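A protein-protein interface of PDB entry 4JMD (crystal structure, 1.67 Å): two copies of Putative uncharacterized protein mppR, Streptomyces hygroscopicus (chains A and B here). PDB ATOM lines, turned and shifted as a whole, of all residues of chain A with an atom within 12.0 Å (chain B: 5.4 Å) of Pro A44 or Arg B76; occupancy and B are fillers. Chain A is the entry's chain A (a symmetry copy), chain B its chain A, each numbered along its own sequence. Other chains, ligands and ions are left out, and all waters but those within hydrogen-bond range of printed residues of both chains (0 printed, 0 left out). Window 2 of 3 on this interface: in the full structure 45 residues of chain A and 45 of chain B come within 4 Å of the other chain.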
ATOM      1  N   GLY A  34      -7.090 -20.456  17.017  1.00  0.00           N
ATOM      2  CA  GLY A  34      -7.723 -19.217  17.432  1.00  0.00           C
ATOM      3  C   GLY A  34      -7.040 -18.045  16.772  1.00  0.00           C
ATOM      4  O   GLY A  34      -6.072 -18.212  16.028  1.00  0.00           O
ATOM      5  N   PRO A  35      -7.553 -16.843  17.023  1.00  0.00           N
ATOM      6  CA  PRO A  35      -6.974 -15.670  16.358  1.00  0.00           C
ATOM      7  C   PRO A  35      -5.597 -15.335  16.906  1.00  0.00           C
ATOM      8  O   PRO A  35      -5.271 -15.671  18.055  1.00  0.00           O
ATOM      9  CB  PRO A  35      -7.992 -14.567  16.646  1.00  0.00           C
ATOM     10  CG  PRO A  35      -8.579 -14.966  17.974  1.00  0.00           C
ATOM     11  CD  PRO A  35      -8.656 -16.480  17.927  1.00  0.00           C
ATOM     12  N   VAL A  36      -4.787 -14.711  16.059  1.00  0.00           N
ATOM     13  CA  VAL A  36      -3.388 -14.469  16.352  1.00  0.00           C
ATOM     14  C   VAL A  36      -3.005 -13.007  16.120  1.00  0.00           C
ATOM     15  O   VAL A  36      -3.802 -12.194  15.624  1.00  0.00           O
ATOM     16  CB  VAL A  36      -2.507 -15.390  15.482  1.00  0.00           C
ATOM     17  CG1 VAL A  36      -2.824 -16.854  15.762  1.00  0.00           C
ATOM     18  CG2 VAL A  36      -2.716 -15.094  14.005  1.00  0.00           C
ATOM     19  N   GLY A  37      -1.777 -12.650  16.477  1.00  0.00           N
ATOM     20  CA  GLY A  37      -1.278 -11.325  16.150  1.00  0.00           C
ATOM     21  C   GLY A  37      -0.104 -10.963  17.024  1.00  0.00           C
ATOM     22  O   GLY A  37      -0.002 -11.428  18.165  1.00  0.00           O
ATOM     23  N   TYR A  38       0.745 -10.069  16.523  1.00  0.00           N
ATOM     24  CA  TYR A  38       1.861  -9.567  17.319  1.00  0.00           C
ATOM     25  C   TYR A  38       1.346  -8.818  18.533  1.00  0.00           C
ATOM     26  O   TYR A  38       1.958  -8.871  19.595  1.00  0.00           O
ATOM     27  CB  TYR A  38       2.753  -8.663  16.477  1.00  0.00           C
ATOM     28  CG  TYR A  38       3.867  -8.036  17.268  1.00  0.00           C
ATOM     29  CD1 TYR A  38       4.945  -8.807  17.735  1.00  0.00           C
ATOM     30  CD2 TYR A  38       3.856  -6.690  17.549  1.00  0.00           C
ATOM     31  CE1 TYR A  38       5.964  -8.224  18.469  1.00  0.00           C
ATOM     32  CE2 TYR A  38       4.866  -6.110  18.297  1.00  0.00           C
ATOM     33  CZ  TYR A  38       5.911  -6.867  18.747  1.00  0.00           C
ATOM     34  OH  TYR A  38       6.920  -6.276  19.486  1.00  0.00           O
ATOM     35  N   SER A  39       0.197  -8.153  18.370  1.00  0.00           N
ATOM     36  CA  SER A  39      -0.458  -7.419  19.434  1.00  0.00           C
ATOM     37  C   SER A  39      -1.962  -7.508  19.228  1.00  0.00           C
ATOM     38  O   SER A  39      -2.431  -8.006  18.209  1.00  0.00           O
ATOM     39  CB  SER A  39      -0.044  -5.942  19.443  1.00  0.00           C
ATOM     40  OG  SER A  39      -0.700  -5.147  18.437  1.00  0.00           O
ATOM     41  N   LEU A  40      -2.698  -6.974  20.192  1.00  0.00           N
ATOM     42  CA  LEU A  40      -4.132  -6.752  20.025  1.00  0.00           C
ATOM     43  C   LEU A  40      -4.381  -5.771  18.882  1.00  0.00           C
ATOM     44  O   LEU A  40      -3.531  -4.927  18.571  1.00  0.00           O
ATOM     45  CB  LEU A  40      -4.733  -6.180  21.299  1.00  0.00           C
ATOM     46  CG  LEU A  40      -4.628  -7.045  22.548  1.00  0.00           C
ATOM     47  CD1 LEU A  40      -5.295  -6.320  23.735  1.00  0.00           C
ATOM     48  CD2 LEU A  40      -5.266  -8.412  22.347  1.00  0.00           C
ATOM     49  N   PRO A  41      -5.556  -5.838  18.255  1.00  0.00           N
ATOM     50  CA  PRO A  41      -6.547  -6.915  18.356  1.00  0.00           C
ATOM     51  C   PRO A  41      -6.066  -8.178  17.653  1.00  0.00           C
ATOM     52  O   PRO A  41      -5.484  -8.098  16.561  1.00  0.00           O
ATOM     53  CB  PRO A  41      -7.774  -6.356  17.613  1.00  0.00           C
ATOM     54  CG  PRO A  41      -7.349  -5.152  16.928  1.00  0.00           C
ATOM     55  CD  PRO A  41      -5.949  -4.772  17.322  1.00  0.00           C
ATOM     56  N   LEU A  42      -6.344  -9.329  18.241  1.00  0.00           N
ATOM     57  CA  LEU A  42      -6.087 -10.602  17.576  1.00  0.00           C
ATOM     58  C   LEU A  42      -7.060 -10.799  16.406  1.00  0.00           C
ATOM     59  O   LEU A  42      -8.199 -10.289  16.419  1.00  0.00           O
ATOM     60  CB  LEU A  42      -6.238 -11.752  18.573  1.00  0.00           C
ATOM     61  CG  LEU A  42      -5.387 -11.700  19.843  1.00  0.00           C
ATOM     62  CD1 LEU A  42      -5.714 -12.877  20.758  1.00  0.00           C
ATOM     63  CD2 LEU A  42      -3.918 -11.678  19.497  1.00  0.00           C
ATOM     64  N   SER A  43      -6.624 -11.523  15.377  1.00  0.00           N
ATOM     65  CA  SER A  43      -7.511 -11.762  14.240  1.00  0.00           C
ATOM     66  C   SER A  43      -7.101 -13.056  13.543  1.00  0.00           C
ATOM     67  O   SER A  43      -6.017 -13.556  13.768  1.00  0.00           O
ATOM     68  CB  SER A  43      -7.479 -10.590  13.255  1.00  0.00           C
ATOM     69  OG  SER A  43      -6.173 -10.393  12.754  1.00  0.00           O
ATOM     70  N   PRO A  44      -7.978 -13.602  12.705  1.00  0.00           N
ATOM     71  CA  PRO A  44      -7.662 -14.915  12.123  1.00  0.00           C
ATOM     72  C   PRO A  44      -6.357 -14.962  11.345  1.00  0.00           C
ATOM     73  O   PRO A  44      -5.670 -15.993  11.429  1.00  0.00           O
ATOM     74  CB  PRO A  44      -8.856 -15.178  11.208  1.00  0.00           C
ATOM     75  CG  PRO A  44      -9.964 -14.498  11.892  1.00  0.00           C
ATOM     76  CD  PRO A  44      -9.368 -13.222  12.431  1.00  0.00           C
ATOM     77  N   THR A  45      -6.021 -13.912  10.596  1.00  0.00           N
ATOM     78  CA  THR A  45      -4.756 -13.893   9.864  1.00  0.00           C
ATOM     79  C   THR A  45      -3.597 -13.170  10.559  1.00  0.00           C
ATOM     80  O   THR A  45      -2.456 -13.240  10.100  1.00  0.00           O
ATOM     81  CB  THR A  45      -4.924 -13.211   8.482  1.00  0.00           C
ATOM     82  OG1 THR A  45      -5.135 -11.811   8.663  1.00  0.00           O
ATOM     83  CG2 THR A  45      -6.095 -13.807   7.734  1.00  0.00           C
ATOM     84  N   GLY A  46      -3.880 -12.453  11.643  1.00  0.00           N
ATOM     85  CA  GLY A  46      -2.877 -11.634  12.297  1.00  0.00           C
ATOM     86  C   GLY A  46      -2.713 -10.244  11.704  1.00  0.00           C
ATOM     87  O   GLY A  46      -1.899  -9.455  12.180  1.00  0.00           O
ATOM     88  N   GLU A  47      -3.513  -9.907  10.690  1.00  0.00           N
ATOM     89  CA  GLU A  47      -3.317  -8.647   9.979  1.00  0.00           C
ATOM     90  C   GLU A  47      -3.865  -7.452  10.771  1.00  0.00           C
ATOM     91  O   GLU A  47      -3.405  -6.339  10.572  1.00  0.00           O
ATOM     92  CB  GLU A  47      -4.002  -8.669   8.615  1.00  0.00           C
ATOM     93  CG  GLU A  47      -5.493  -8.513   8.733  1.00  0.00           C
ATOM     94  CD  GLU A  47      -6.182  -8.122   7.444  1.00  0.00           C
ATOM     95  OE1 GLU A  47      -5.554  -8.200   6.357  1.00  0.00           O
ATOM     96  OE2 GLU A  47      -7.368  -7.735   7.536  1.00  0.00           O
ATOM     97  N   SER A  48      -4.821  -7.695  11.672  1.00  0.00           N
ATOM     98  CA  SER A  48      -5.487  -6.599  12.411  1.00  0.00           C
ATOM     99  C   SER A  48      -4.643  -5.971  13.521  1.00  0.00           C
ATOM    100  O   SER A  48      -4.968  -4.889  13.985  1.00  0.00           O
ATOM    101  CB  SER A  48      -6.824  -7.058  13.017  1.00  0.00           C
ATOM    102  OG  SER A  48      -7.778  -7.416  12.016  1.00  0.00           O
ATOM    103  N   ALA A  49      -3.589  -6.654  13.959  1.00  0.00           N
ATOM    104  CA  ALA A  49      -2.758  -6.166  15.085  1.00  0.00           C
ATOM    105  C   ALA A  49      -2.383  -4.704  14.950  1.00  0.00           C
ATOM    106  O   ALA A  49      -1.929  -4.283  13.903  1.00  0.00           O
ATOM    107  CB  ALA A  49      -1.489  -6.995  15.173  1.00  0.00           C
ATOM    108  N   MET A  50      -2.546  -3.949  16.024  1.00  0.00           N
ATOM    109  CA  MET A  50      -2.171  -2.537  16.016  1.00  0.00           C
ATOM    110  C   MET A  50      -0.668  -2.325  15.729  1.00  0.00           C
ATOM    111  O   MET A  50      -0.298  -1.378  14.995  1.00  0.00           O
ATOM    112  CB  MET A  50      -2.551  -1.892  17.358  1.00  0.00           C
ATOM    113  CG  MET A  50      -2.523  -0.372  17.290  1.00  0.00           C
ATOM    114  SD  MET A  50      -2.976   0.326  18.872  1.00  0.00           S
ATOM    115  CE  MET A  50      -1.368   0.293  19.490  1.00  0.00           C
ATOM    116  N   PRO B  71     -21.735 -16.784  11.432  1.00  0.00           N
ATOM    117  CA  PRO B  71     -21.264 -17.442  12.659  1.00  0.00           C
ATOM    118  C   PRO B  71     -19.876 -18.067  12.518  1.00  0.00           C
ATOM    119  O   PRO B  71     -19.140 -18.154  13.507  1.00  0.00           O
ATOM    120  CB  PRO B  71     -22.295 -18.557  12.890  1.00  0.00           C
ATOM    121  CG  PRO B  71     -23.466 -18.217  12.053  1.00  0.00           C
ATOM    122  CD  PRO B  71     -22.983 -17.367  10.919  1.00  0.00           C
ATOM    123  N   ASP B  72     -19.538 -18.478  11.294  1.00  0.00           N
ATOM    124  CA  ASP B  72     -18.247 -19.083  10.971  1.00  0.00           C
ATOM    125  C   ASP B  72     -17.117 -18.043  10.992  1.00  0.00           C
ATOM    126  O   ASP B  72     -15.963 -18.375  11.268  1.00  0.00           O
ATOM    127  CB  ASP B  72     -18.304 -19.757   9.595  1.00  0.00           C
ATOM    128  CG  ASP B  72     -19.300 -20.913   9.538  1.00  0.00           C
ATOM    129  OD1 ASP B  72     -19.521 -21.583  10.566  1.00  0.00           O
ATOM    130  OD2 ASP B  72     -19.859 -21.157   8.448  1.00  0.00           O
ATOM    131  N   ALA B  73     -17.457 -16.799  10.674  1.00  0.00           N
ATOM    132  CA  ALA B  73     -16.527 -15.668  10.830  1.00  0.00           C
ATOM    133  C   ALA B  73     -16.318 -15.335  12.296  1.00  0.00           C
ATOM    134  O   ALA B  73     -15.191 -15.123  12.736  1.00  0.00           O
ATOM    135  CB  ALA B  73     -17.017 -14.439  10.079  1.00  0.00           C
ATOM    136  N   ALA B  74     -17.406 -15.261  13.053  1.00  0.00           N
ATOM    137  CA  ALA B  74     -17.328 -14.968  14.476  1.00  0.00           C
ATOM    138  C   ALA B  74     -16.505 -16.004  15.253  1.00  0.00           C
ATOM    139  O   ALA B  74     -15.693 -15.639  16.114  1.00  0.00           O
ATOM    140  CB  ALA B  74     -18.733 -14.842  15.063  1.00  0.00           C
ATOM    141  N   ARG B  75     -16.720 -17.279  14.943  1.00  0.00           N
ATOM    142  CA  ARG B  75     -16.007 -18.388  15.578  1.00  0.00           C
ATOM    143  C   ARG B  75     -14.491 -18.215  15.473  1.00  0.00           C
ATOM    144  O   ARG B  75     -13.759 -18.522  16.420  1.00  0.00           O
ATOM    145  CB  ARG B  75     -16.448 -19.724  14.954  1.00  0.00           C
ATOM    146  CG  ARG B  75     -15.635 -20.933  15.389  1.00  0.00           C
ATOM    147  CD  ARG B  75     -16.047 -22.204  14.633  1.00  0.00           C
ATOM    148  NE  ARG B  75     -15.824 -22.105  13.188  1.00  0.00           N
ATOM    149  CZ  ARG B  75     -14.635 -22.215  12.594  1.00  0.00           C
ATOM    150  NH1 ARG B  75     -13.539 -22.431  13.309  1.00  0.00           N
ATOM    151  NH2 ARG B  75     -14.536 -22.109  11.275  1.00  0.00           N
ATOM    152  N   ARG B  76     -14.023 -17.711  14.336  1.00  0.00           N
ATOM    153  CA  ARG B  76     -12.585 -17.532  14.102  1.00  0.00           C
ATOM    154  C   ARG B  76     -11.966 -16.407  14.938  1.00  0.00           C
ATOM    155  O   ARG B  76     -10.716 -16.335  15.043  1.00  0.00           O
ATOM    156  CB  ARG B  76     -12.306 -17.280  12.613  1.00  0.00           C
ATOM    157  CG  ARG B  76     -12.648 -18.451  11.708  1.00  0.00           C
ATOM    158  CD  ARG B  76     -12.510 -18.054  10.234  1.00  0.00           C
ATOM    159  NE  ARG B  76     -11.116 -18.051   9.788  1.00  0.00           N
ATOM    160  CZ  ARG B  76     -10.613 -17.257   8.840  1.00  0.00           C
ATOM    161  NH1 ARG B  76     -11.376 -16.362   8.217  1.00  0.00           N
ATOM    162  NH2 ARG B  76      -9.326 -17.350   8.515  1.00  0.00           N
ATOM    163  N   PHE B  77     -12.808 -15.553  15.528  1.00  0.00           N
ATOM    164  CA  PHE B  77     -12.325 -14.523  16.458  1.00  0.00           C
ATOM    165  C   PHE B  77     -12.340 -14.980  17.931  1.00  0.00           C
ATOM    166  O   PHE B  77     -11.918 -14.251  18.839  1.00  0.00           O
ATOM    167  CB  PHE B  77     -13.145 -13.238  16.291  1.00  0.00           C
ATOM    168  CG  PHE B  77     -12.683 -12.372  15.154  1.00  0.00           C
ATOM    169  CD1 PHE B  77     -11.681 -11.431  15.339  1.00  0.00           C
ATOM    170  CD2 PHE B  77     -13.241 -12.500  13.902  1.00  0.00           C
ATOM    171  CE1 PHE B  77     -11.269 -10.635  14.281  1.00  0.00           C
ATOM    172  CE2 PHE B  77     -12.831 -11.716  12.849  1.00  0.00           C
ATOM    173  CZ  PHE B  77     -11.840 -10.771  13.036  1.00  0.00           C
ATOM    174  N   LEU B  78     -12.854 -16.180  18.194  1.00  0.00           N
ATOM    175  CA  LEU B  78     -12.924 -16.652  19.573  1.00  0.00           C
ATOM    176  C   LEU B  78     -11.693 -17.473  19.922  1.00  0.00           C
ATOM    177  O   LEU B  78     -11.389 -18.475  19.249  1.00  0.00           O
ATOM    178  CB  LEU B  78     -14.176 -17.503  19.796  1.00  0.00           C
ATOM    179  CG  LEU B  78     -15.506 -16.818  19.477  1.00  0.00           C
ATOM    180  CD1 LEU B  78     -16.598 -17.838  19.734  1.00  0.00           C
ATOM    181  CD2 LEU B  78     -15.744 -15.563  20.293  1.00  0.00           C
ATOM    182  N   ASP B 264     -10.099  -9.016   7.501  1.00  0.00           N
ATOM    183  CA  ASP B 264     -10.439  -9.717   8.736  1.00  0.00           C
ATOM    184  C   ASP B 264     -11.607  -9.015   9.428  1.00  0.00           C
ATOM    185  O   ASP B 264     -12.581  -9.652   9.816  1.00  0.00           O
ATOM    186  CB  ASP B 264      -9.224  -9.843   9.668  1.00  0.00           C
ATOM    187  CG  ASP B 264      -8.359 -11.064   9.340  1.00  0.00           C
ATOM    188  OD1 ASP B 264      -8.865 -11.983   8.662  1.00  0.00           O
ATOM    189  OD2 ASP B 264      -7.185 -11.113   9.767  1.00  0.00           O
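The backbone NH (N) of Val A36 sits at hydrogen-bond distance from the backbone carbonyl oxygen (O) of Ser A43, 2.8 Å away. The side-chain hydroxyl of Ser A43 lies within hydrogen-bond range of the backbone NH of Gly A46 (3.3 Å). The backbone NH (N) of Glu A47 sits at hydrogen-bond distance from the side-chain hydroxyl (OG) of Ser A43 (3.4 Å). The side-chain hydroxyl (OG) of Ser A43 is in hydrogen-bond range of the backbone NH (N) of Ser A48, at 3.2 Å. OG1 of Thr A45 lies within hydrogen-bond range of N of Glu A47, at 3.2 Å.
CD of Pro A35 touches O of Arg B76, 3.5 Å away. Phe B77 touches Pro A35 (O to CG, 3.5 Å). Pro A35 touches Leu B78. Phe B77 touches Leu A42. Ser A43 touches Phe B77. Arg B76 touches Pro A44 (NH2 to CB, 3.5 Å). Pro A44 touches Phe B77. Pro A44 touches Asp B264 (CD to CG, 3.9 Å). CB of Asp B264 touches OG of Ser A48, 3.7 Å away.
Gly A34 touches none of the printed residues of chain B. Pro A41 touches none of the printed residues of chain B. Of the printed residues of chain B, Leu A42 touches Phe B77 (3.8 Å). Of the printed residues of chain B, Ser A43 touches Phe B77 (3.9 Å) and Asp B264 (3.2 Å). Printed residues of chain B within 4 Å of Pro A44: Arg B76 (3.5 Å), Phe B77 (3.5 Å) and Asp B264 (3.9 Å). Of the printed residues of chain B, Ser A48 touches Asp B264. No residue of chain A comes within 4 Å of Ala B73. No residue of chain A comes within 4 Å of Ala B74. No residue of chain A comes within 4 Å of Arg B75. Arg B76 touches two residues of chain A. The nearest printed residue of chain B that does not touch Pro A44 is Ala B73 (5.3 Å). The nearest residue of chain A that does not touch Arg B76 is Gly A34 (4.4 Å).
The side-chain carboxylate (OD2) of Asp B264 is in hydrogen-bond range of the side-chain hydroxyl (OG) of Ser A43. OD2 of Asp B264 is in hydrogen-bond range of OG1 of Thr A45 (2.4 Å). N of Asp B264 lies within hydrogen-bond range of OE2 of Glu A47, at 3.0 Å.
No position is printed for both chains.
Of the 17 printed residues of chain A, 7 touch a printed residue of chain B. Hydrophobic or aromatic side chains of chain A within 4 Å of the printed part of chain B: Pro A35 and Pro A44.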
